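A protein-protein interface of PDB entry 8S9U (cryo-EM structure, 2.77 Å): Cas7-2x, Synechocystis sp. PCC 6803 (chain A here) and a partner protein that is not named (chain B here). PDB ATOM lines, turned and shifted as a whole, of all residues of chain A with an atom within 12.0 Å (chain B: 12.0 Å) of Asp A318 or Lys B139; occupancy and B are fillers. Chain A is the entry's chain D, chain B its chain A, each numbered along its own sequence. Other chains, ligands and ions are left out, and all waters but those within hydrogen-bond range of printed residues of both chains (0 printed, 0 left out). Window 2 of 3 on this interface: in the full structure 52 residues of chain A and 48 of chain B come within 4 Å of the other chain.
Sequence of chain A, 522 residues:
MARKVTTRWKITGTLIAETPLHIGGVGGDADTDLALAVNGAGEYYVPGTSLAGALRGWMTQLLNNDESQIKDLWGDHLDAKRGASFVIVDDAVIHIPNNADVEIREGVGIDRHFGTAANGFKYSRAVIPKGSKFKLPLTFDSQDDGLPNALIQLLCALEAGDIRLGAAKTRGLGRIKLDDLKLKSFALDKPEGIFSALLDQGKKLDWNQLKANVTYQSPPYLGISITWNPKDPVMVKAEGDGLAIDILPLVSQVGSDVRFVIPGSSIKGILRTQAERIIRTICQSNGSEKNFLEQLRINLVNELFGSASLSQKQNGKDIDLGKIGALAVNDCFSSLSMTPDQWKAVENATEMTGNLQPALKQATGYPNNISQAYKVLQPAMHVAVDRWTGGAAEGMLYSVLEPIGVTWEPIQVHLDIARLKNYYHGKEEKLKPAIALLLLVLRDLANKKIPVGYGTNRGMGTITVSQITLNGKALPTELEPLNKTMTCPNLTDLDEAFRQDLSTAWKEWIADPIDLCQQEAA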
ATOM      1  N   HIS A  77     -21.556  -0.684 -22.441  1.00  0.00           N
ATOM      2  CA  HIS A  77     -21.518   0.291 -23.521  1.00  0.00           C
ATOM      3  C   HIS A  77     -20.118   0.774 -23.878  1.00  0.00           C
ATOM      4  O   HIS A  77     -19.886   1.150 -25.030  1.00  0.00           O
ATOM      5  CB  HIS A  77     -22.409   1.486 -23.188  1.00  0.00           C
ATOM      6  CG  HIS A  77     -22.182   2.077 -21.833  1.00  0.00           C
ATOM      7  ND1 HIS A  77     -21.959   1.318 -20.707  1.00  0.00           N
ATOM      8  CD2 HIS A  77     -22.186   3.363 -21.419  1.00  0.00           C
ATOM      9  CE1 HIS A  77     -21.811   2.110 -19.664  1.00  0.00           C
ATOM     10  NE2 HIS A  77     -21.943   3.358 -20.069  1.00  0.00           N
ATOM     11  N   ALA A 308     -35.559  10.223   1.203  1.00  0.00           N
ATOM     12  CA  ALA A 308     -35.971  10.540  -0.153  1.00  0.00           C
ATOM     13  C   ALA A 308     -34.769  10.899  -1.003  1.00  0.00           C
ATOM     14  O   ALA A 308     -33.849  11.577  -0.543  1.00  0.00           O
ATOM     15  CB  ALA A 308     -36.962  11.698  -0.150  1.00  0.00           C
ATOM     16  N   SER A 309     -34.812  10.495  -2.270  1.00  0.00           N
ATOM     17  CA  SER A 309     -33.851  10.995  -3.237  1.00  0.00           C
ATOM     18  C   SER A 309     -33.955  12.506  -3.297  1.00  0.00           C
ATOM     19  O   SER A 309     -35.045  13.056  -3.451  1.00  0.00           O
ATOM     20  CB  SER A 309     -34.110  10.386  -4.612  1.00  0.00           C
ATOM     21  OG  SER A 309     -33.694   9.038  -4.683  1.00  0.00           O
ATOM     22  N   LEU A 310     -32.820  13.179  -3.142  1.00  0.00           N
ATOM     23  CA  LEU A 310     -32.819  14.639  -3.169  1.00  0.00           C
ATOM     24  C   LEU A 310     -31.394  15.085  -3.513  1.00  0.00           C
ATOM     25  O   LEU A 310     -30.550  15.219  -2.630  1.00  0.00           O
ATOM     26  CB  LEU A 310     -33.283  15.202  -1.846  1.00  0.00           C
ATOM     27  CG  LEU A 310     -33.194  16.697  -1.599  1.00  0.00           C
ATOM     28  CD1 LEU A 310     -33.967  17.414  -2.668  1.00  0.00           C
ATOM     29  CD2 LEU A 310     -33.748  17.013  -0.241  1.00  0.00           C
ATOM     30  N   SER A 311     -31.146  15.294  -4.798  1.00  0.00           N
ATOM     31  CA  SER A 311     -29.856  15.808  -5.227  1.00  0.00           C
ATOM     32  C   SER A 311     -29.636  17.228  -4.722  1.00  0.00           C
ATOM     33  O   SER A 311     -30.489  18.102  -4.898  1.00  0.00           O
ATOM     34  CB  SER A 311     -29.744  15.773  -6.749  1.00  0.00           C
ATOM     35  OG  SER A 311     -30.846  16.415  -7.352  1.00  0.00           O
ATOM     36  N   GLN A 312     -28.480  17.456  -4.104  1.00  0.00           N
ATOM     37  CA  GLN A 312     -28.120  18.759  -3.575  1.00  0.00           C
ATOM     38  C   GLN A 312     -26.683  19.047  -3.968  1.00  0.00           C
ATOM     39  O   GLN A 312     -25.819  18.176  -3.862  1.00  0.00           O
ATOM     40  CB  GLN A 312     -28.259  18.819  -2.048  1.00  0.00           C
ATOM     41  CG  GLN A 312     -29.667  18.629  -1.505  1.00  0.00           C
ATOM     42  CD  GLN A 312     -30.598  19.808  -1.767  1.00  0.00           C
ATOM     43  OE1 GLN A 312     -30.386  20.604  -2.683  1.00  0.00           O
ATOM     44  NE2 GLN A 312     -31.636  19.924  -0.950  1.00  0.00           N
ATOM     45  N   LYS A 313     -26.434  20.269  -4.425  1.00  0.00           N
ATOM     46  CA  LYS A 313     -25.075  20.760  -4.619  1.00  0.00           C
ATOM     47  C   LYS A 313     -24.438  21.065  -3.270  1.00  0.00           C
ATOM     48  O   LYS A 313     -24.848  22.003  -2.579  1.00  0.00           O
ATOM     49  CB  LYS A 313     -25.085  21.991  -5.514  1.00  0.00           C
ATOM     50  CG  LYS A 313     -25.550  21.705  -6.924  1.00  0.00           C
ATOM     51  CD  LYS A 313     -24.425  21.123  -7.755  1.00  0.00           C
ATOM     52  CE  LYS A 313     -23.390  22.184  -8.087  1.00  0.00           C
ATOM     53  NZ  LYS A 313     -22.363  21.675  -9.035  1.00  0.00           N
ATOM     54  N   GLN A 314     -23.435  20.276  -2.889  1.00  0.00           N
ATOM     55  CA  GLN A 314     -22.779  20.471  -1.602  1.00  0.00           C
ATOM     56  C   GLN A 314     -21.778  21.617  -1.671  1.00  0.00           C
ATOM     57  O   GLN A 314     -21.917  22.625  -0.969  1.00  0.00           O
ATOM     58  CB  GLN A 314     -22.090  19.179  -1.163  1.00  0.00           C
ATOM     59  CG  GLN A 314     -21.489  19.239   0.222  1.00  0.00           C
ATOM     60  CD  GLN A 314     -20.961  17.897   0.677  1.00  0.00           C
ATOM     61  OE1 GLN A 314     -20.690  17.016  -0.137  1.00  0.00           O
ATOM     62  NE2 GLN A 314     -20.810  17.734   1.985  1.00  0.00           N
ATOM     63  N   ASN A 315     -20.755  21.472  -2.514  1.00  0.00           N
ATOM     64  CA  ASN A 315     -19.926  22.607  -2.921  1.00  0.00           C
ATOM     65  C   ASN A 315     -19.190  22.173  -4.193  1.00  0.00           C
ATOM     66  O   ASN A 315     -18.130  21.552  -4.124  1.00  0.00           O
ATOM     67  CB  ASN A 315     -18.958  23.020  -1.831  1.00  0.00           C
ATOM     68  CG  ASN A 315     -18.146  24.244  -2.204  1.00  0.00           C
ATOM     69  OD1 ASN A 315     -18.516  24.999  -3.102  1.00  0.00           O
ATOM     70  ND2 ASN A 315     -17.032  24.447  -1.512  1.00  0.00           N
ATOM     71  N   GLY A 316     -19.768  22.516  -5.342  1.00  0.00           N
ATOM     72  CA  GLY A 316     -19.322  21.966  -6.607  1.00  0.00           C
ATOM     73  C   GLY A 316     -19.764  20.531  -6.790  1.00  0.00           C
ATOM     74  O   GLY A 316     -20.457  20.199  -7.754  1.00  0.00           O
ATOM     75  N   LYS A 317     -19.353  19.670  -5.865  1.00  0.00           N
ATOM     76  CA  LYS A 317     -19.820  18.291  -5.840  1.00  0.00           C
ATOM     77  C   LYS A 317     -21.336  18.248  -5.698  1.00  0.00           C
ATOM     78  O   LYS A 317     -21.938  19.092  -5.030  1.00  0.00           O
ATOM     79  CB  LYS A 317     -19.150  17.532  -4.692  1.00  0.00           C
ATOM     80  CG  LYS A 317     -19.517  16.064  -4.593  1.00  0.00           C
ATOM     81  CD  LYS A 317     -18.830  15.410  -3.407  1.00  0.00           C
ATOM     82  CE  LYS A 317     -19.145  13.925  -3.330  1.00  0.00           C
ATOM     83  NZ  LYS A 317     -18.397  13.256  -2.232  1.00  0.00           N
ATOM     84  N   ASP A 318     -21.953  17.261  -6.337  1.00  0.00           N
ATOM     85  CA  ASP A 318     -23.392  17.058  -6.275  1.00  0.00           C
ATOM     86  C   ASP A 318     -23.640  15.697  -5.644  1.00  0.00           C
ATOM     87  O   ASP A 318     -23.052  14.699  -6.068  1.00  0.00           O
ATOM     88  CB  ASP A 318     -24.006  17.139  -7.675  1.00  0.00           C
ATOM     89  CG  ASP A 318     -25.525  17.132  -7.660  1.00  0.00           C
ATOM     90  OD1 ASP A 318     -26.127  16.716  -6.650  1.00  0.00           O
ATOM     91  OD2 ASP A 318     -26.121  17.551  -8.672  1.00  0.00           O
ATOM     92  N   ILE A 319     -24.508  15.658  -4.635  1.00  0.00           N
ATOM     93  CA  ILE A 319     -24.722  14.462  -3.833  1.00  0.00           C
ATOM     94  C   ILE A 319     -26.212  14.182  -3.717  1.00  0.00           C
ATOM     95  O   ILE A 319     -27.013  15.098  -3.509  1.00  0.00           O
ATOM     96  CB  ILE A 319     -24.102  14.619  -2.430  1.00  0.00           C
ATOM     97  CG1 ILE A 319     -24.640  15.879  -1.750  1.00  0.00           C
ATOM     98  CG2 ILE A 319     -22.595  14.687  -2.519  1.00  0.00           C
ATOM     99  CD1 ILE A 319     -24.298  15.983  -0.295  1.00  0.00           C
ATOM    100  N   ASP A 320     -26.584  12.917  -3.875  1.00  0.00           N
ATOM    101  CA  ASP A 320     -27.922  12.467  -3.524  1.00  0.00           C
ATOM    102  C   ASP A 320     -27.999  12.237  -2.020  1.00  0.00           C
ATOM    103  O   ASP A 320     -27.250  11.424  -1.473  1.00  0.00           O
ATOM    104  CB  ASP A 320     -28.266  11.192  -4.286  1.00  0.00           C
ATOM    105  CG  ASP A 320     -29.727  10.822  -4.170  1.00  0.00           C
ATOM    106  OD1 ASP A 320     -30.531  11.692  -3.793  1.00  0.00           O
ATOM    107  OD2 ASP A 320     -30.072   9.656  -4.452  1.00  0.00           O
ATOM    108  N   LEU A 321     -28.894  12.960  -1.350  1.00  0.00           N
ATOM    109  CA  LEU A 321     -29.257  12.647   0.027  1.00  0.00           C
ATOM    110  C   LEU A 321     -30.123  11.399   0.151  1.00  0.00           C
ATOM    111  O   LEU A 321     -30.258  10.863   1.254  1.00  0.00           O
ATOM    112  CB  LEU A 321     -29.972  13.842   0.654  1.00  0.00           C
ATOM    113  CG  LEU A 321     -29.122  14.972   1.238  1.00  0.00           C
ATOM    114  CD1 LEU A 321     -28.078  15.484   0.272  1.00  0.00           C
ATOM    115  CD2 LEU A 321     -30.027  16.104   1.656  1.00  0.00           C
ATOM    116  N   GLY A 322     -30.704  10.926  -0.943  1.00  0.00           N
ATOM    117  CA  GLY A 322     -31.542   9.746  -0.883  1.00  0.00           C
ATOM    118  C   GLY A 322     -30.764   8.462  -0.702  1.00  0.00           C
ATOM    119  O   GLY A 322     -29.694   8.271  -1.279  1.00  0.00           O
ATOM    120  N   LYS A 323     -31.303   7.578   0.128  1.00  0.00           N
ATOM    121  CA  LYS A 323     -30.880   6.192   0.100  1.00  0.00           C
ATOM    122  C   LYS A 323     -32.062   5.298   0.443  1.00  0.00           C
ATOM    123  O   LYS A 323     -32.948   5.680   1.203  1.00  0.00           O
ATOM    124  CB  LYS A 323     -29.706   5.922   1.040  1.00  0.00           C
ATOM    125  CG  LYS A 323     -29.998   6.013   2.498  1.00  0.00           C
ATOM    126  CD  LYS A 323     -28.725   6.326   3.238  1.00  0.00           C
ATOM    127  CE  LYS A 323     -28.291   7.744   2.988  1.00  0.00           C
ATOM    128  NZ  LYS A 323     -27.003   8.032   3.640  1.00  0.00           N
ATOM    129  N   GLN A 518     -21.423   9.896   6.729  1.00  0.00           N
ATOM    130  CA  GLN A 518     -20.438  10.843   6.235  1.00  0.00           C
ATOM    131  C   GLN A 518     -19.053  10.472   6.740  1.00  0.00           C
ATOM    132  O   GLN A 518     -18.881  10.082   7.898  1.00  0.00           O
ATOM    133  CB  GLN A 518     -20.807  12.258   6.672  1.00  0.00           C
ATOM    134  CG  GLN A 518     -19.955  13.338   6.059  1.00  0.00           C
ATOM    135  CD  GLN A 518     -20.557  14.712   6.251  1.00  0.00           C
ATOM    136  OE1 GLN A 518     -21.461  14.896   7.066  1.00  0.00           O
ATOM    137  NE2 GLN A 518     -20.064  15.686   5.498  1.00  0.00           N
ATOM    138  N   GLY B 127     -37.728   4.660 -18.180  1.00  0.00           N
ATOM    139  CA  GLY B 127     -36.428   4.061 -17.969  1.00  0.00           C
ATOM    140  C   GLY B 127     -35.589   4.832 -16.980  1.00  0.00           C
ATOM    141  O   GLY B 127     -35.370   6.028 -17.155  1.00  0.00           O
ATOM    142  N   VAL B 128     -35.115   4.168 -15.935  1.00  0.00           N
ATOM    143  CA  VAL B 128     -34.291   4.806 -14.922  1.00  0.00           C
ATOM    144  C   VAL B 128     -33.175   3.856 -14.524  1.00  0.00           C
ATOM    145  O   VAL B 128     -33.339   2.633 -14.526  1.00  0.00           O
ATOM    146  CB  VAL B 128     -35.127   5.222 -13.691  1.00  0.00           C
ATOM    147  CG1 VAL B 128     -35.482   4.019 -12.829  1.00  0.00           C
ATOM    148  CG2 VAL B 128     -34.412   6.278 -12.890  1.00  0.00           C
ATOM    149  N   ALA B 129     -32.031   4.426 -14.170  1.00  0.00           N
ATOM    150  CA  ALA B 129     -30.893   3.660 -13.695  1.00  0.00           C
ATOM    151  C   ALA B 129     -30.775   3.899 -12.206  1.00  0.00           C
ATOM    152  O   ALA B 129     -30.843   5.040 -11.749  1.00  0.00           O
ATOM    153  CB  ALA B 129     -29.602   4.056 -14.405  1.00  0.00           C
ATOM    154  N   ILE B 130     -30.612   2.833 -11.468  1.00  0.00           N
ATOM    155  CA  ILE B 130     -30.521   2.881 -10.020  1.00  0.00           C
ATOM    156  C   ILE B 130     -29.070   2.821  -9.572  1.00  0.00           C
ATOM    157  O   ILE B 130     -28.257   2.082 -10.137  1.00  0.00           O
ATOM    158  CB  ILE B 130     -31.367   1.750  -9.416  1.00  0.00           C
ATOM    159  CG1 ILE B 130     -32.832   2.173  -9.438  1.00  0.00           C
ATOM    160  CG2 ILE B 130     -30.881   1.353  -8.048  1.00  0.00           C
ATOM    161  CD1 ILE B 130     -33.751   1.104  -9.044  1.00  0.00           C
ATOM    162  N   ASP B 131     -28.747   3.622  -8.559  1.00  0.00           N
ATOM    163  CA  ASP B 131     -27.429   3.603  -7.949  1.00  0.00           C
ATOM    164  C   ASP B 131     -27.262   2.347  -7.106  1.00  0.00           C
ATOM    165  O   ASP B 131     -28.099   2.040  -6.259  1.00  0.00           O
ATOM    166  CB  ASP B 131     -27.241   4.842  -7.094  1.00  0.00           C
ATOM    167  CG  ASP B 131     -25.808   5.072  -6.739  1.00  0.00           C
ATOM    168  OD1 ASP B 131     -25.268   4.274  -5.955  1.00  0.00           O
ATOM    169  OD2 ASP B 131     -25.219   6.050  -7.243  1.00  0.00           O
ATOM    170  N   ALA B 132     -26.172   1.617  -7.340  1.00  0.00           N
ATOM    171  CA  ALA B 132     -26.009   0.300  -6.734  1.00  0.00           C
ATOM    172  C   ALA B 132     -25.819   0.342  -5.225  1.00  0.00           C
ATOM    173  O   ALA B 132     -26.204  -0.606  -4.536  1.00  0.00           O
ATOM    174  CB  ALA B 132     -24.829  -0.422  -7.377  1.00  0.00           C
ATOM    175  N   ILE B 133     -25.221   1.399  -4.687  1.00  0.00           N
ATOM    176  CA  ILE B 133     -25.045   1.483  -3.241  1.00  0.00           C
ATOM    177  C   ILE B 133     -26.246   2.111  -2.545  1.00  0.00           C
ATOM    178  O   ILE B 133     -26.705   1.599  -1.526  1.00  0.00           O
ATOM    179  CB  ILE B 133     -23.731   2.224  -2.913  1.00  0.00           C
ATOM    180  CG1 ILE B 133     -23.781   3.678  -3.385  1.00  0.00           C
ATOM    181  CG2 ILE B 133     -22.549   1.491  -3.520  1.00  0.00           C
ATOM    182  CD1 ILE B 133     -22.725   4.566  -2.787  1.00  0.00           C
ATOM    183  N   THR B 134     -26.796   3.205  -3.071  1.00  0.00           N
ATOM    184  CA  THR B 134     -27.938   3.842  -2.430  1.00  0.00           C
ATOM    185  C   THR B 134     -29.257   3.164  -2.755  1.00  0.00           C
ATOM    186  O   THR B 134     -30.225   3.351  -2.018  1.00  0.00           O
ATOM    187  CB  THR B 134     -28.019   5.310  -2.820  1.00  0.00           C
ATOM    188  OG1 THR B 134     -28.452   5.418  -4.173  1.00  0.00           O
ATOM    189  CG2 THR B 134     -26.674   5.955  -2.685  1.00  0.00           C
ATOM    190  N   GLY B 135     -29.324   2.389  -3.829  1.00  0.00           N
ATOM    191  CA  GLY B 135     -30.585   1.841  -4.280  1.00  0.00           C
ATOM    192  C   GLY B 135     -31.573   2.854  -4.798  1.00  0.00           C
ATOM    193  O   GLY B 135     -32.761   2.554  -4.879  1.00  0.00           O
ATOM    194  N   THR B 136     -31.117   4.048  -5.149  1.00  0.00           N
ATOM    195  CA  THR B 136     -31.975   5.112  -5.633  1.00  0.00           C
ATOM    196  C   THR B 136     -31.586   5.481  -7.056  1.00  0.00           C
ATOM    197  O   THR B 136     -30.494   5.164  -7.529  1.00  0.00           O
ATOM    198  CB  THR B 136     -31.922   6.347  -4.725  1.00  0.00           C
ATOM    199  OG1 THR B 136     -30.659   7.001  -4.863  1.00  0.00           O
ATOM    200  CG2 THR B 136     -32.109   5.942  -3.300  1.00  0.00           C
ATOM    201  N   ALA B 137     -32.508   6.151  -7.739  1.00  0.00           N
ATOM    202  CA  ALA B 137     -32.266   6.636  -9.088  1.00  0.00           C
ATOM    203  C   ALA B 137     -31.009   7.481  -9.173  1.00  0.00           C
ATOM    204  O   ALA B 137     -30.823   8.417  -8.394  1.00  0.00           O
ATOM    205  CB  ALA B 137     -33.466   7.453  -9.553  1.00  0.00           C
ATOM    206  N   LYS B 138     -30.146   7.147 -10.133  1.00  0.00           N
ATOM    207  CA  LYS B 138     -29.007   7.996 -10.453  1.00  0.00           C
ATOM    208  C   LYS B 138     -29.487   9.333 -10.990  1.00  0.00           C
ATOM    209  O   LYS B 138     -30.528   9.426 -11.639  1.00  0.00           O
ATOM    210  CB  LYS B 138     -28.121   7.333 -11.494  1.00  0.00           C
ATOM    211  CG  LYS B 138     -27.417   6.099 -11.036  1.00  0.00           C
ATOM    212  CD  LYS B 138     -26.500   5.613 -12.120  1.00  0.00           C
ATOM    213  CE  LYS B 138     -25.712   4.423 -11.668  1.00  0.00           C
ATOM    214  NZ  LYS B 138     -24.737   4.016 -12.706  1.00  0.00           N
ATOM    215  N   LYS B 139     -28.708  10.376 -10.738  1.00  0.00           N
ATOM    216  CA  LYS B 139     -28.919  11.617 -11.461  1.00  0.00           C
ATOM    217  C   LYS B 139     -28.673  11.402 -12.947  1.00  0.00           C
ATOM    218  O   LYS B 139     -27.855  10.572 -13.342  1.00  0.00           O
ATOM    219  CB  LYS B 139     -28.007  12.714 -10.925  1.00  0.00           C
ATOM    220  CG  LYS B 139     -28.425  14.093 -11.368  1.00  0.00           C
ATOM    221  CD  LYS B 139     -27.356  15.115 -11.119  1.00  0.00           C
ATOM    222  CE  LYS B 139     -27.796  16.470 -11.622  1.00  0.00           C
ATOM    223  NZ  LYS B 139     -26.723  17.490 -11.464  1.00  0.00           N
ATOM    224  N   ASP B 140     -29.408  12.156 -13.768  1.00  0.00           N
ATOM    225  CA  ASP B 140     -29.275  12.194 -15.222  1.00  0.00           C
ATOM    226  C   ASP B 140     -29.931  10.997 -15.891  1.00  0.00           C
ATOM    227  O   ASP B 140     -30.458  11.113 -16.996  1.00  0.00           O
ATOM    228  CB  ASP B 140     -27.813  12.273 -15.657  1.00  0.00           C
ATOM    229  CG  ASP B 140     -27.225  13.642 -15.476  1.00  0.00           C
ATOM    230  OD1 ASP B 140     -27.995  14.602 -15.270  1.00  0.00           O
ATOM    231  OD2 ASP B 140     -25.987  13.764 -15.553  1.00  0.00           O
ATOM    232  N   PHE B 141     -29.919   9.851 -15.228  1.00  0.00           N
ATOM    233  CA  PHE B 141     -30.277   8.584 -15.855  1.00  0.00           C
ATOM    234  C   PHE B 141     -31.781   8.328 -15.794  1.00  0.00           C
ATOM    235  O   PHE B 141     -32.246   7.350 -15.222  1.00  0.00           O
ATOM    236  CB  PHE B 141     -29.509   7.448 -15.192  1.00  0.00           C
ATOM    237  CG  PHE B 141     -28.043   7.411 -15.524  1.00  0.00           C
ATOM    238  CD1 PHE B 141     -27.240   8.503 -15.317  1.00  0.00           C
ATOM    239  CD2 PHE B 141     -27.466   6.261 -16.006  1.00  0.00           C
ATOM    240  CE1 PHE B 141     -25.914   8.464 -15.610  1.00  0.00           C
ATOM    241  CE2 PHE B 141     -26.130   6.218 -16.296  1.00  0.00           C
ATOM    242  CZ  PHE B 141     -25.357   7.323 -16.097  1.00  0.00           C
ATOM    243  N   LEU B 142     -32.544   9.232 -16.400  1.00  0.00           N
ATOM    244  CA  LEU B 142     -33.991   9.090 -16.522  1.00  0.00           C
ATOM    245  C   LEU B 142     -34.375   9.319 -17.969  1.00  0.00           C
ATOM    246  O   LEU B 142     -34.169  10.409 -18.503  1.00  0.00           O
ATOM    247  CB  LEU B 142     -34.741  10.062 -15.611  1.00  0.00           C
ATOM    248  CG  LEU B 142     -36.253   9.851 -15.584  1.00  0.00           C
ATOM    249  CD1 LEU B 142     -36.607   8.500 -15.029  1.00  0.00           C
ATOM    250  CD2 LEU B 142     -36.882  10.933 -14.784  1.00  0.00           C
ATOM    251  N   ARG B 143     -34.985   8.317 -18.582  1.00  0.00           N
ATOM    252  CA  ARG B 143     -35.322   8.365 -19.989  1.00  0.00           C
ATOM    253  C   ARG B 143     -36.740   7.876 -20.190  1.00  0.00           C
ATOM    254  O   ARG B 143     -37.275   7.101 -19.398  1.00  0.00           O
ATOM    255  CB  ARG B 143     -34.375   7.498 -20.810  1.00  0.00           C
ATOM    256  CG  ARG B 143     -34.530   6.038 -20.502  1.00  0.00           C
ATOM    257  CD  ARG B 143     -33.464   5.194 -21.104  1.00  0.00           C
ATOM    258  NE  ARG B 143     -33.697   3.796 -20.786  1.00  0.00           N
ATOM    259  CZ  ARG B 143     -33.279   3.215 -19.674  1.00  0.00           C
ATOM    260  NH1 ARG B 143     -32.605   3.922 -18.784  1.00  0.00           N
ATOM    261  NH2 ARG B 143     -33.537   1.935 -19.450  1.00  0.00           N
ATOM    262  N   PHE B 144     -37.335   8.328 -21.283  1.00  0.00           N
ATOM    263  CA  PHE B 144     -38.661   7.905 -21.700  1.00  0.00           C
ATOM    264  C   PHE B 144     -38.552   7.528 -23.164  1.00  0.00           C
ATOM    265  O   PHE B 144     -38.093   8.329 -23.981  1.00  0.00           O
ATOM    266  CB  PHE B 144     -39.688   9.000 -21.432  1.00  0.00           C
ATOM    267  CG  PHE B 144     -39.905   9.230 -19.971  1.00  0.00           C
ATOM    268  CD1 PHE B 144     -40.660   8.345 -19.226  1.00  0.00           C
ATOM    269  CD2 PHE B 144     -39.281  10.273 -19.323  1.00  0.00           C
ATOM    270  CE1 PHE B 144     -40.828   8.527 -17.885  1.00  0.00           C
ATOM    271  CE2 PHE B 144     -39.449  10.455 -17.983  1.00  0.00           C
ATOM    272  CZ  PHE B 144     -40.224   9.580 -17.263  1.00  0.00           C
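Thr B136 touches Ser A309.
CB of Thr B134 touches O of Gly A322 (3.7 Å).
C of Gly A322 touches CG2 of Thr B136, at 3.9 Å.
Lys A323 touches Thr B134.
Lys A323 touches Thr B136 (CA to CG2, 3.6 Å).
The side-chain carboxylate of Asp B131 is in hydrogen-bond range of the backbone NH of Thr B134 (3.4 Å).
The backbone NH (N) of Gly A322 sits at hydrogen-bond distance from the side-chain carboxylate (OD1) of Asp A320 (3.0 Å).
The backbone carbonyl oxygen (O) of Ala A308 lies close to the backbone NH (N) of Gly A322, at 3.2 Å.
O of Thr B136 lies within hydrogen-bond range of N of Asp B131 (2.5 Å).
N of Leu A310 sits at hydrogen-bond distance from OD1 of Asp A320, 2.8 Å away.
The side-chain hydroxyl (OG1) of Thr B134 is in hydrogen-bond range of the side-chain hydroxyl (OG1) of Thr B136 (2.8 Å).
Of the printed residues of chain B, Ser A309 touches Thr B136 (3.2 Å).
Leu A310 touches none of the printed residues of chain B.
No residue of chain B comes within 4 Å of Ser A311.
No residue of chain B comes within 4 Å of Gly A316.
Of chain B, only Lys B139 comes within 4 Å of Asp A318.
No residue of chain B comes within 4 Å of Ile A319.
Of chain B, only Thr B136 comes within 4 Å of Asp A320.
Of the printed residues of chain B, Gly A322 touches Thr B134 (3.7 Å) and Thr B136 (3.9 Å).
No residue of chain A comes within 4 Å of Ala B129.
Printed residues of chain A within 4 Å of Thr B134: Gly A322 and Lys A323.
Of the printed residues of chain A, Thr B136 touches Ser A309, Asp A320, Gly A322 and Lys A323.
Lys B139 touches just one residue of chain A: Asp A318 (2.9 Å).
No residue of chain A comes within 4 Å of Asp B140.
No residue of chain A comes within 4 Å of Phe B141.
The nearest residue of chain A that does not touch Lys B139 is Ser A311 (5.0 Å).
The nearest printed residue of chain A that does not touch Thr B134 is Asp A320 (4.5 Å).
The side-chain carboxylate of Asp A320 lies within hydrogen-bond range of the side-chain hydroxyl of Thr B136, at 2.8 Å.
The side-chain amino group (NZ) of Lys B139 lies within salt-bridge range of the side-chain carboxylate (OD2) of Asp A318, 2.9 Å away.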
